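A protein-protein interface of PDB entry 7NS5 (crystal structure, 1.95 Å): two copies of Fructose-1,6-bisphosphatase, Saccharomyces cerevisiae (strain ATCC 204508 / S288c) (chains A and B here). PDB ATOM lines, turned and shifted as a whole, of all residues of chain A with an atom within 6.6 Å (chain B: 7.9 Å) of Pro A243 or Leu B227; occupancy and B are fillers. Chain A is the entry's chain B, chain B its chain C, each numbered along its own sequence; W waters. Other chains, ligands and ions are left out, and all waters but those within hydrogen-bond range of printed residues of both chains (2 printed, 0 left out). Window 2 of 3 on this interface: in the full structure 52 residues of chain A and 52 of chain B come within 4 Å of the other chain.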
ATOM      1  N   LYS A 239      24.087  25.194  -2.284  1.00  0.00           N
ATOM      2  CA  LYS A 239      22.954  26.061  -1.944  1.00  0.00           C
ATOM      3  C   LYS A 239      21.630  25.300  -1.905  1.00  0.00           C
ATOM      4  O   LYS A 239      20.758  25.598  -1.078  1.00  0.00           O
ATOM      5  CB  LYS A 239      22.841  27.218  -2.936  1.00  0.00           C
ATOM      6  CG  LYS A 239      23.577  28.470  -2.489  1.00  0.00           C
ATOM      7  CD  LYS A 239      23.396  29.633  -3.475  1.00  0.00           C
ATOM      8  CE  LYS A 239      24.652  30.492  -3.641  1.00  0.00           C
ATOM      9  NZ  LYS A 239      24.459  31.503  -4.746  1.00  0.00           N
ATOM     10  N   VAL A 240      21.435  24.325  -2.801  1.00  0.00           N
ATOM     11  CA  VAL A 240      20.119  23.694  -2.863  1.00  0.00           C
ATOM     12  C   VAL A 240      19.873  22.789  -1.664  1.00  0.00           C
ATOM     13  O   VAL A 240      18.721  22.420  -1.407  1.00  0.00           O
ATOM     14  CB  VAL A 240      19.927  22.908  -4.178  1.00  0.00           C
ATOM     15  CG1 VAL A 240      20.124  23.816  -5.387  1.00  0.00           C
ATOM     16  CG2 VAL A 240      20.879  21.745  -4.253  1.00  0.00           C
ATOM     17  N   LYS A 241      20.928  22.406  -0.936  1.00  0.00           N
ATOM     18  CA  LYS A 241      20.820  21.623   0.296  1.00  0.00           C
ATOM     19  C   LYS A 241      20.475  22.448   1.529  1.00  0.00           C
ATOM     20  O   LYS A 241      20.198  21.861   2.582  1.00  0.00           O
ATOM     21  CB  LYS A 241      22.129  20.889   0.555  1.00  0.00           C
ATOM     22  CG  LYS A 241      22.440  19.890  -0.553  1.00  0.00           C
ATOM     23  CD  LYS A 241      23.771  19.174  -0.312  1.00  0.00           C
ATOM     24  CE  LYS A 241      24.168  18.477  -1.586  1.00  0.00           C
ATOM     25  NZ  LYS A 241      25.261  17.501  -1.365  1.00  0.00           N
ATOM     26  N   GLN A 242      20.519  23.767   1.439  1.00  0.00           N
ATOM     27  CA  GLN A 242      20.130  24.651   2.532  1.00  0.00           C
ATOM     28  C   GLN A 242      18.617  24.809   2.621  1.00  0.00           C
ATOM     29  O   GLN A 242      17.901  24.545   1.655  1.00  0.00           O
ATOM     30  CB  GLN A 242      20.778  26.022   2.352  1.00  0.00           C
ATOM     31  CG  GLN A 242      22.227  25.976   1.979  1.00  0.00           C
ATOM     32  CD  GLN A 242      23.106  25.758   3.193  1.00  0.00           C
ATOM     33  OE1 GLN A 242      22.611  25.478   4.294  1.00  0.00           O
ATOM     34  NE2 GLN A 242      24.412  25.927   3.016  1.00  0.00           N
ATOM     35  N   PRO A 243      18.105  25.264   3.767  1.00  0.00           N
ATOM     36  CA  PRO A 243      16.668  25.564   3.854  1.00  0.00           C
ATOM     37  C   PRO A 243      16.285  26.595   2.803  1.00  0.00           C
ATOM     38  O   PRO A 243      17.051  27.508   2.502  1.00  0.00           O
ATOM     39  CB  PRO A 243      16.492  26.116   5.278  1.00  0.00           C
ATOM     40  CG  PRO A 243      17.734  25.755   6.022  1.00  0.00           C
ATOM     41  CD  PRO A 243      18.828  25.548   5.023  1.00  0.00           C
ATOM     42  N   GLN A 244      15.105  26.426   2.214  1.00  0.00           N
ATOM     43  CA  GLN A 244      14.632  27.332   1.174  1.00  0.00           C
ATOM     44  C   GLN A 244      13.350  28.001   1.643  1.00  0.00           C
ATOM     45  O   GLN A 244      12.368  27.313   1.943  1.00  0.00           O
ATOM     46  CB  GLN A 244      14.384  26.600  -0.146  1.00  0.00           C
ATOM     47  CG  GLN A 244      15.531  25.733  -0.625  1.00  0.00           C
ATOM     48  CD  GLN A 244      16.643  26.545  -1.241  1.00  0.00           C
ATOM     49  OE1 GLN A 244      16.419  27.298  -2.184  1.00  0.00           O
ATOM     50  NE2 GLN A 244      17.861  26.370  -0.735  1.00  0.00           N
ATOM     51  N   ALA A 245      13.339  29.331   1.645  1.00  0.00           N
ATOM     52  CA  ALA A 245      12.146  30.068   2.116  1.00  0.00           C
ATOM     53  C   ALA A 245      10.939  29.704   1.248  1.00  0.00           C
ATOM     54  O   ALA A 245       9.848  29.503   1.811  1.00  0.00           O
ATOM     55  CB  ALA A 245      12.417  31.546   2.094  1.00  0.00           C
ATOM     56  N   ASN A 247      10.119  27.115   0.063  1.00  0.00           N
ATOM     57  CA  ASN A 247       9.816  25.697   0.194  1.00  0.00           C
ATOM     58  C   ASN A 247       9.533  25.358   1.656  1.00  0.00           C
ATOM     59  O   ASN A 247       9.759  24.228   2.103  1.00  0.00           O
ATOM     60  CB  ASN A 247      10.960  24.853  -0.377  1.00  0.00           C
ATOM     61  CG  ASN A 247      10.689  23.359  -0.314  1.00  0.00           C
ATOM     62  OD1 ASN A 247       9.579  22.906  -0.577  1.00  0.00           O
ATOM     63  ND2 ASN A 247      11.713  22.587   0.050  1.00  0.00           N
ATOM     64  N   ASN A 248       9.033  26.345   2.416  1.00  0.00           N
ATOM     65  CA  ASN A 248       8.732  26.191   3.845  1.00  0.00           C
ATOM     66  C   ASN A 248       9.988  25.881   4.648  1.00  0.00           C
ATOM     67  O   ASN A 248       9.981  25.018   5.528  1.00  0.00           O
ATOM     68  CB  ASN A 248       7.670  25.117   4.096  1.00  0.00           C
ATOM     69  CG  ASN A 248       6.543  25.161   3.091  1.00  0.00           C
ATOM     70  OD1 ASN A 248       6.153  26.234   2.620  1.00  0.00           O
ATOM     71  ND2 ASN A 248       6.017  23.990   2.745  1.00  0.00           N
ATOM     72  N   ASN A 249      11.075  26.581   4.342  1.00  0.00           N
ATOM     73  CA  ASN A 249      12.341  26.436   5.057  1.00  0.00           C
ATOM     74  C   ASN A 249      12.889  25.012   4.972  1.00  0.00           C
ATOM     75  O   ASN A 249      13.676  24.585   5.825  1.00  0.00           O
ATOM     76  CB  ASN A 249      12.191  26.870   6.522  1.00  0.00           C
ATOM     77  CG  ASN A 249      13.521  27.056   7.218  1.00  0.00           C
ATOM     78  OD1 ASN A 249      13.892  26.256   8.077  1.00  0.00           O
ATOM     79  ND2 ASN A 249      14.251  28.114   6.849  1.00  0.00           N
ATOM     80  N   LYS A 250      12.478  24.267   3.968  1.00  0.00           N
ATOM     81  CA  LYS A 250      12.995  22.927   3.774  1.00  0.00           C
ATOM     82  C   LYS A 250      14.017  22.931   2.643  1.00  0.00           C
ATOM     83  O   LYS A 250      13.902  23.713   1.696  1.00  0.00           O
ATOM     84  CB  LYS A 250      11.859  21.978   3.409  1.00  0.00           C
ATOM     85  CG  LYS A 250      10.822  21.788   4.502  1.00  0.00           C
ATOM     86  CD  LYS A 250       9.902  20.654   4.136  1.00  0.00           C
ATOM     87  CE  LYS A 250       8.600  21.246   3.504  1.00  0.00           C
ATOM     88  NZ  LYS A 250       8.205  20.798   2.109  1.00  0.00           N
ATOM     89  N   PRO A 251      15.025  22.072   2.676  1.00  0.00           N
ATOM     90  CA  PRO A 251      15.983  22.024   1.563  1.00  0.00           C
ATOM     91  C   PRO A 251      15.362  21.349   0.349  1.00  0.00           C
ATOM     92  O   PRO A 251      14.262  20.794   0.408  1.00  0.00           O
ATOM     93  CB  PRO A 251      17.143  21.201   2.120  1.00  0.00           C
ATOM     94  CG  PRO A 251      16.493  20.316   3.166  1.00  0.00           C
ATOM     95  CD  PRO A 251      15.344  21.095   3.736  1.00  0.00           C
ATOM     96  N   PHE A 252      16.076  21.414  -0.777  1.00  0.00           N
ATOM     97  CA  PHE A 252      15.640  20.652  -1.948  1.00  0.00           C
ATOM     98  C   PHE A 252      15.663  19.160  -1.646  1.00  0.00           C
ATOM     99  O   PHE A 252      16.464  18.684  -0.834  1.00  0.00           O
ATOM    100  CB  PHE A 252      16.545  20.869  -3.157  1.00  0.00           C
ATOM    101  CG  PHE A 252      16.273  22.127  -3.949  1.00  0.00           C
ATOM    102  CD1 PHE A 252      16.264  23.362  -3.342  1.00  0.00           C
ATOM    103  CD2 PHE A 252      16.063  22.055  -5.328  1.00  0.00           C
ATOM    104  CE1 PHE A 252      16.053  24.508  -4.073  1.00  0.00           C
ATOM    105  CE2 PHE A 252      15.851  23.191  -6.071  1.00  0.00           C
ATOM    106  CZ  PHE A 252      15.852  24.429  -5.442  1.00  0.00           C
ATOM    107  N   ASN B 222      19.393  10.037  -0.476  1.00  0.00           N
ATOM    108  CA  ASN B 222      18.750  11.319  -0.770  1.00  0.00           C
ATOM    109  C   ASN B 222      19.573  12.429  -0.128  1.00  0.00           C
ATOM    110  O   ASN B 222      19.393  12.744   1.052  1.00  0.00           O
ATOM    111  CB  ASN B 222      17.308  11.323  -0.252  1.00  0.00           C
ATOM    112  CG  ASN B 222      16.581  12.615  -0.563  1.00  0.00           C
ATOM    113  OD1 ASN B 222      17.173  13.548  -1.108  1.00  0.00           O
ATOM    114  ND2 ASN B 222      15.290  12.687  -0.202  1.00  0.00           N
ATOM    115  N   GLU B 223      20.468  13.050  -0.904  1.00  0.00           N
ATOM    116  CA  GLU B 223      21.371  14.035  -0.314  1.00  0.00           C
ATOM    117  C   GLU B 223      20.680  15.374  -0.093  1.00  0.00           C
ATOM    118  O   GLU B 223      21.285  16.289   0.471  1.00  0.00           O
ATOM    119  CB  GLU B 223      22.630  14.203  -1.178  1.00  0.00           C
ATOM    120  CG  GLU B 223      23.666  13.080  -1.060  1.00  0.00           C
ATOM    121  CD  GLU B 223      25.039  13.491  -1.640  1.00  0.00           C
ATOM    122  OE1 GLU B 223      25.680  14.388  -1.075  1.00  0.00           O
ATOM    123  OE2 GLU B 223      25.467  12.931  -2.685  1.00  0.00           O
ATOM    124  N   GLY B 224      19.418  15.508  -0.501  1.00  0.00           N
ATOM    125  CA  GLY B 224      18.603  16.588   0.030  1.00  0.00           C
ATOM    126  C   GLY B 224      18.418  16.525   1.535  1.00  0.00           C
ATOM    127  O   GLY B 224      18.056  17.533   2.148  1.00  0.00           O
ATOM    128  N   ASN B 225      18.650  15.368   2.149  1.00  0.00           N
ATOM    129  CA  ASN B 225      18.516  15.260   3.597  1.00  0.00           C
ATOM    130  C   ASN B 225      19.820  15.571   4.335  1.00  0.00           C
ATOM    131  O   ASN B 225      19.884  15.402   5.557  1.00  0.00           O
ATOM    132  CB  ASN B 225      17.973  13.875   3.972  1.00  0.00           C
ATOM    133  CG  ASN B 225      16.496  13.704   3.563  1.00  0.00           C
ATOM    134  OD1 ASN B 225      15.759  14.682   3.507  1.00  0.00           O
ATOM    135  ND2 ASN B 225      16.086  12.481   3.239  1.00  0.00           N
ATOM    136  N   THR B 226      20.840  16.050   3.618  1.00  0.00           N
ATOM    137  CA  THR B 226      22.126  16.362   4.245  1.00  0.00           C
ATOM    138  C   THR B 226      21.968  17.267   5.465  1.00  0.00           C
ATOM    139  O   THR B 226      22.574  17.018   6.515  1.00  0.00           O
ATOM    140  CB  THR B 226      23.054  17.005   3.220  1.00  0.00           C
ATOM    141  OG1 THR B 226      23.336  16.046   2.196  1.00  0.00           O
ATOM    142  CG2 THR B 226      24.377  17.458   3.898  1.00  0.00           C
ATOM    143  N   LEU B 227      21.136  18.305   5.344  1.00  0.00           N
ATOM    144  CA  LEU B 227      20.871  19.246   6.433  1.00  0.00           C
ATOM    145  C   LEU B 227      20.459  18.551   7.730  1.00  0.00           C
ATOM    146  O   LEU B 227      20.685  19.084   8.822  1.00  0.00           O
ATOM    147  CB  LEU B 227      19.762  20.220   6.001  1.00  0.00           C
ATOM    148  CG  LEU B 227      19.382  21.348   6.965  1.00  0.00           C
ATOM    149  CD1 LEU B 227      20.571  22.284   7.110  1.00  0.00           C
ATOM    150  CD2 LEU B 227      18.137  22.102   6.502  1.00  0.00           C
ATOM    151  N   TYR B 228      19.830  17.380   7.634  1.00  0.00           N
ATOM    152  CA  TYR B 228      19.271  16.703   8.796  1.00  0.00           C
ATOM    153  C   TYR B 228      20.122  15.535   9.273  1.00  0.00           C
ATOM    154  O   TYR B 228      19.746  14.870  10.248  1.00  0.00           O
ATOM    155  CB  TYR B 228      17.842  16.211   8.496  1.00  0.00           C
ATOM    156  CG  TYR B 228      16.886  17.270   7.976  1.00  0.00           C
ATOM    157  CD1 TYR B 228      16.330  17.171   6.705  1.00  0.00           C
ATOM    158  CD2 TYR B 228      16.546  18.373   8.753  1.00  0.00           C
ATOM    159  CE1 TYR B 228      15.441  18.133   6.221  1.00  0.00           C
ATOM    160  CE2 TYR B 228      15.675  19.347   8.276  1.00  0.00           C
ATOM    161  CZ  TYR B 228      15.124  19.215   7.002  1.00  0.00           C
ATOM    162  OH  TYR B 228      14.255  20.161   6.514  1.00  0.00           O
ATOM    163  N   TRP B 229      21.256  15.265   8.629  1.00  0.00           N
ATOM    164  CA  TRP B 229      22.118  14.173   9.064  1.00  0.00           C
ATOM    165  C   TRP B 229      23.061  14.650  10.150  1.00  0.00           C
ATOM    166  O   TRP B 229      23.468  15.818  10.166  1.00  0.00           O
ATOM    167  CB  TRP B 229      22.957  13.645   7.902  1.00  0.00           C
ATOM    168  CG  TRP B 229      22.126  12.894   6.912  1.00  0.00           C
ATOM    169  CD1 TRP B 229      20.910  12.299   7.129  1.00  0.00           C
ATOM    170  CD2 TRP B 229      22.427  12.708   5.535  1.00  0.00           C
ATOM    171  NE1 TRP B 229      20.449  11.737   5.958  1.00  0.00           N
ATOM    172  CE2 TRP B 229      21.360  11.980   4.964  1.00  0.00           C
ATOM    173  CE3 TRP B 229      23.504  13.076   4.723  1.00  0.00           C
ATOM    174  CZ2 TRP B 229      21.343  11.612   3.632  1.00  0.00           C
ATOM    175  CZ3 TRP B 229      23.479  12.707   3.386  1.00  0.00           C
ATOM    176  CH2 TRP B 229      22.403  11.995   2.859  1.00  0.00           C
ATOM    177  N   ASN B 230      23.444  13.727  11.035  1.00  0.00           N
ATOM    178  CA  ASN B 230      24.527  14.022  11.963  1.00  0.00           C
ATOM    179  C   ASN B 230      25.868  13.972  11.225  1.00  0.00           C
ATOM    180  O   ASN B 230      25.950  13.639  10.039  1.00  0.00           O
ATOM    181  CB  ASN B 230      24.482  13.088  13.176  1.00  0.00           C
ATOM    182  CG  ASN B 230      24.815  11.629  12.853  1.00  0.00           C
ATOM    183  OD1 ASN B 230      25.584  11.312  11.942  1.00  0.00           O
ATOM    184  ND2 ASN B 230      24.286  10.725  13.679  1.00  0.00           N
ATOM    185  N   ARG B 234      27.070  12.552   7.435  1.00  0.00           N
ATOM    186  CA  ARG B 234      27.521  13.564   6.482  1.00  0.00           C
ATOM    187  C   ARG B 234      28.948  13.299   6.018  1.00  0.00           C
ATOM    188  O   ARG B 234      29.239  13.352   4.820  1.00  0.00           O
ATOM    189  CB  ARG B 234      27.436  14.966   7.100  1.00  0.00           C
ATOM    190  CG  ARG B 234      26.068  15.629   7.040  1.00  0.00           C
ATOM    191  CD  ARG B 234      26.078  16.994   7.752  1.00  0.00           C
ATOM    192  NE  ARG B 234      26.592  18.067   6.894  1.00  0.00           N
ATOM    193  CZ  ARG B 234      25.972  19.237   6.717  1.00  0.00           C
ATOM    194  NH1 ARG B 234      24.824  19.479   7.339  1.00  0.00           N
ATOM    195  NH2 ARG B 234      26.490  20.167   5.922  1.00  0.00           N
ATOM    196  N   ASP B 279      17.448  10.933  10.538  1.00  0.00           N
ATOM    197  CA  ASP B 279      17.656  12.353  10.311  1.00  0.00           C
ATOM    198  C   ASP B 279      16.667  13.099  11.200  1.00  0.00           C
ATOM    199  O   ASP B 279      15.739  12.504  11.754  1.00  0.00           O
ATOM    200  CB  ASP B 279      17.577  12.660   8.802  1.00  0.00           C
ATOM    201  CG  ASP B 279      16.139  12.720   8.234  1.00  0.00           C
ATOM    202  OD1 ASP B 279      15.143  12.964   8.949  1.00  0.00           O
ATOM    203  OD2 ASP B 279      16.010  12.380   7.036  1.00  0.00           O
ATOM    204  N   LYS B 280      16.906  14.405  11.376  1.00  0.00           N
ATOM    205  CA  LYS B 280      16.100  15.180  12.322  1.00  0.00           C
ATOM    206  C   LYS B 280      14.601  15.060  12.075  1.00  0.00           C
ATOM    207  O   LYS B 280      13.811  15.177  13.019  1.00  0.00           O
ATOM    208  CB  LYS B 280      16.497  16.654  12.281  1.00  0.00           C
ATOM    209  CG  LYS B 280      17.862  16.958  12.861  1.00  0.00           C
ATOM    210  CD  LYS B 280      18.046  18.466  13.008  1.00  0.00           C
ATOM    211  CE  LYS B 280      19.521  18.897  12.948  1.00  0.00           C
ATOM    212  NZ  LYS B 280      19.656  20.388  13.039  1.00  0.00           N
HETATM  213  O   HOH W   1      25.760  15.485   1.336  1.00  0.00           O
HETATM  214  O   HOH W   2      20.266  19.140   2.874  1.00  0.00           O
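Water W1 lies within hydrogen-bond range of OG1 of Thr B226 (2.6 Å), OE1 of Glu B223 (2.7 Å) and NZ of Lys A241 (3.4 Å).
Water W2 lies within hydrogen-bond range of the backbone carbonyl oxygen (O) of Lys A241 (2.7 Å), the backbone NH (N) of Leu B227 (2.7 Å), the backbone carbonyl oxygen (O) of Gly B224 (2.8 Å) and the backbone NH (N) of Thr B226 (3.2 Å).
Pro A243 touches just one residue of chain B: Leu B227.
Of the printed residues of chain B, Pro A251 touches Gly B224 (3.4 Å) and Tyr B228 (3.1 Å).
Of chain A, only Lys A241 (3.8 Å) and Pro A243 (3.7 Å) come within 4 Å of Leu B227.
Of the printed residues of chain A, Tyr B228 touches Pro A251 (3.1 Å).
Among the printed residues, merely in contact across the chains: Phe A252 with Gly B224, Pro A251 with Tyr B228, Pro A251 with Gly B224, Pro A243 with Leu B227 and Lys A241 with Leu B227.
No position is printed for both chains.
Of the 6 pairs that touch across the chains among the printed residues, none has its exchanged pair printed and touching as well.
The backbone NH (N) of Phe A252 lies within hydrogen-bond range of the backbone carbonyl oxygen (O) of Val A240, at 2.9 Å.
The backbone carbonyl oxygen of Glu B223 lies within hydrogen-bond range of the side-chain hydroxyl of Thr B226 (2.7 Å).
OD1 of Asn B222 is in hydrogen-bond range of N of Gly B224 (3.0 Å).
The side-chain amide nitrogen of Asn A247 lies within hydrogen-bond range of the backbone carbonyl oxygen of Pro A251.
The backbone carbonyl oxygen of Tyr B228 is in hydrogen-bond range of the backbone NH of Lys B280 (3.1 Å).
Hydrophobic or aromatic side chains of chain A that line the printed part of chain B: Pro A243 and Pro A251.
Printed residues of chain B that touch a printed residue of chain A: Glu B223, Gly B224, Leu B227 and Tyr B228.
Among the printed residues, 6 pairs touch across the chains.
OE1 of Glu B223 is in salt-bridge range of NZ of Lys A241 (3.2 Å).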
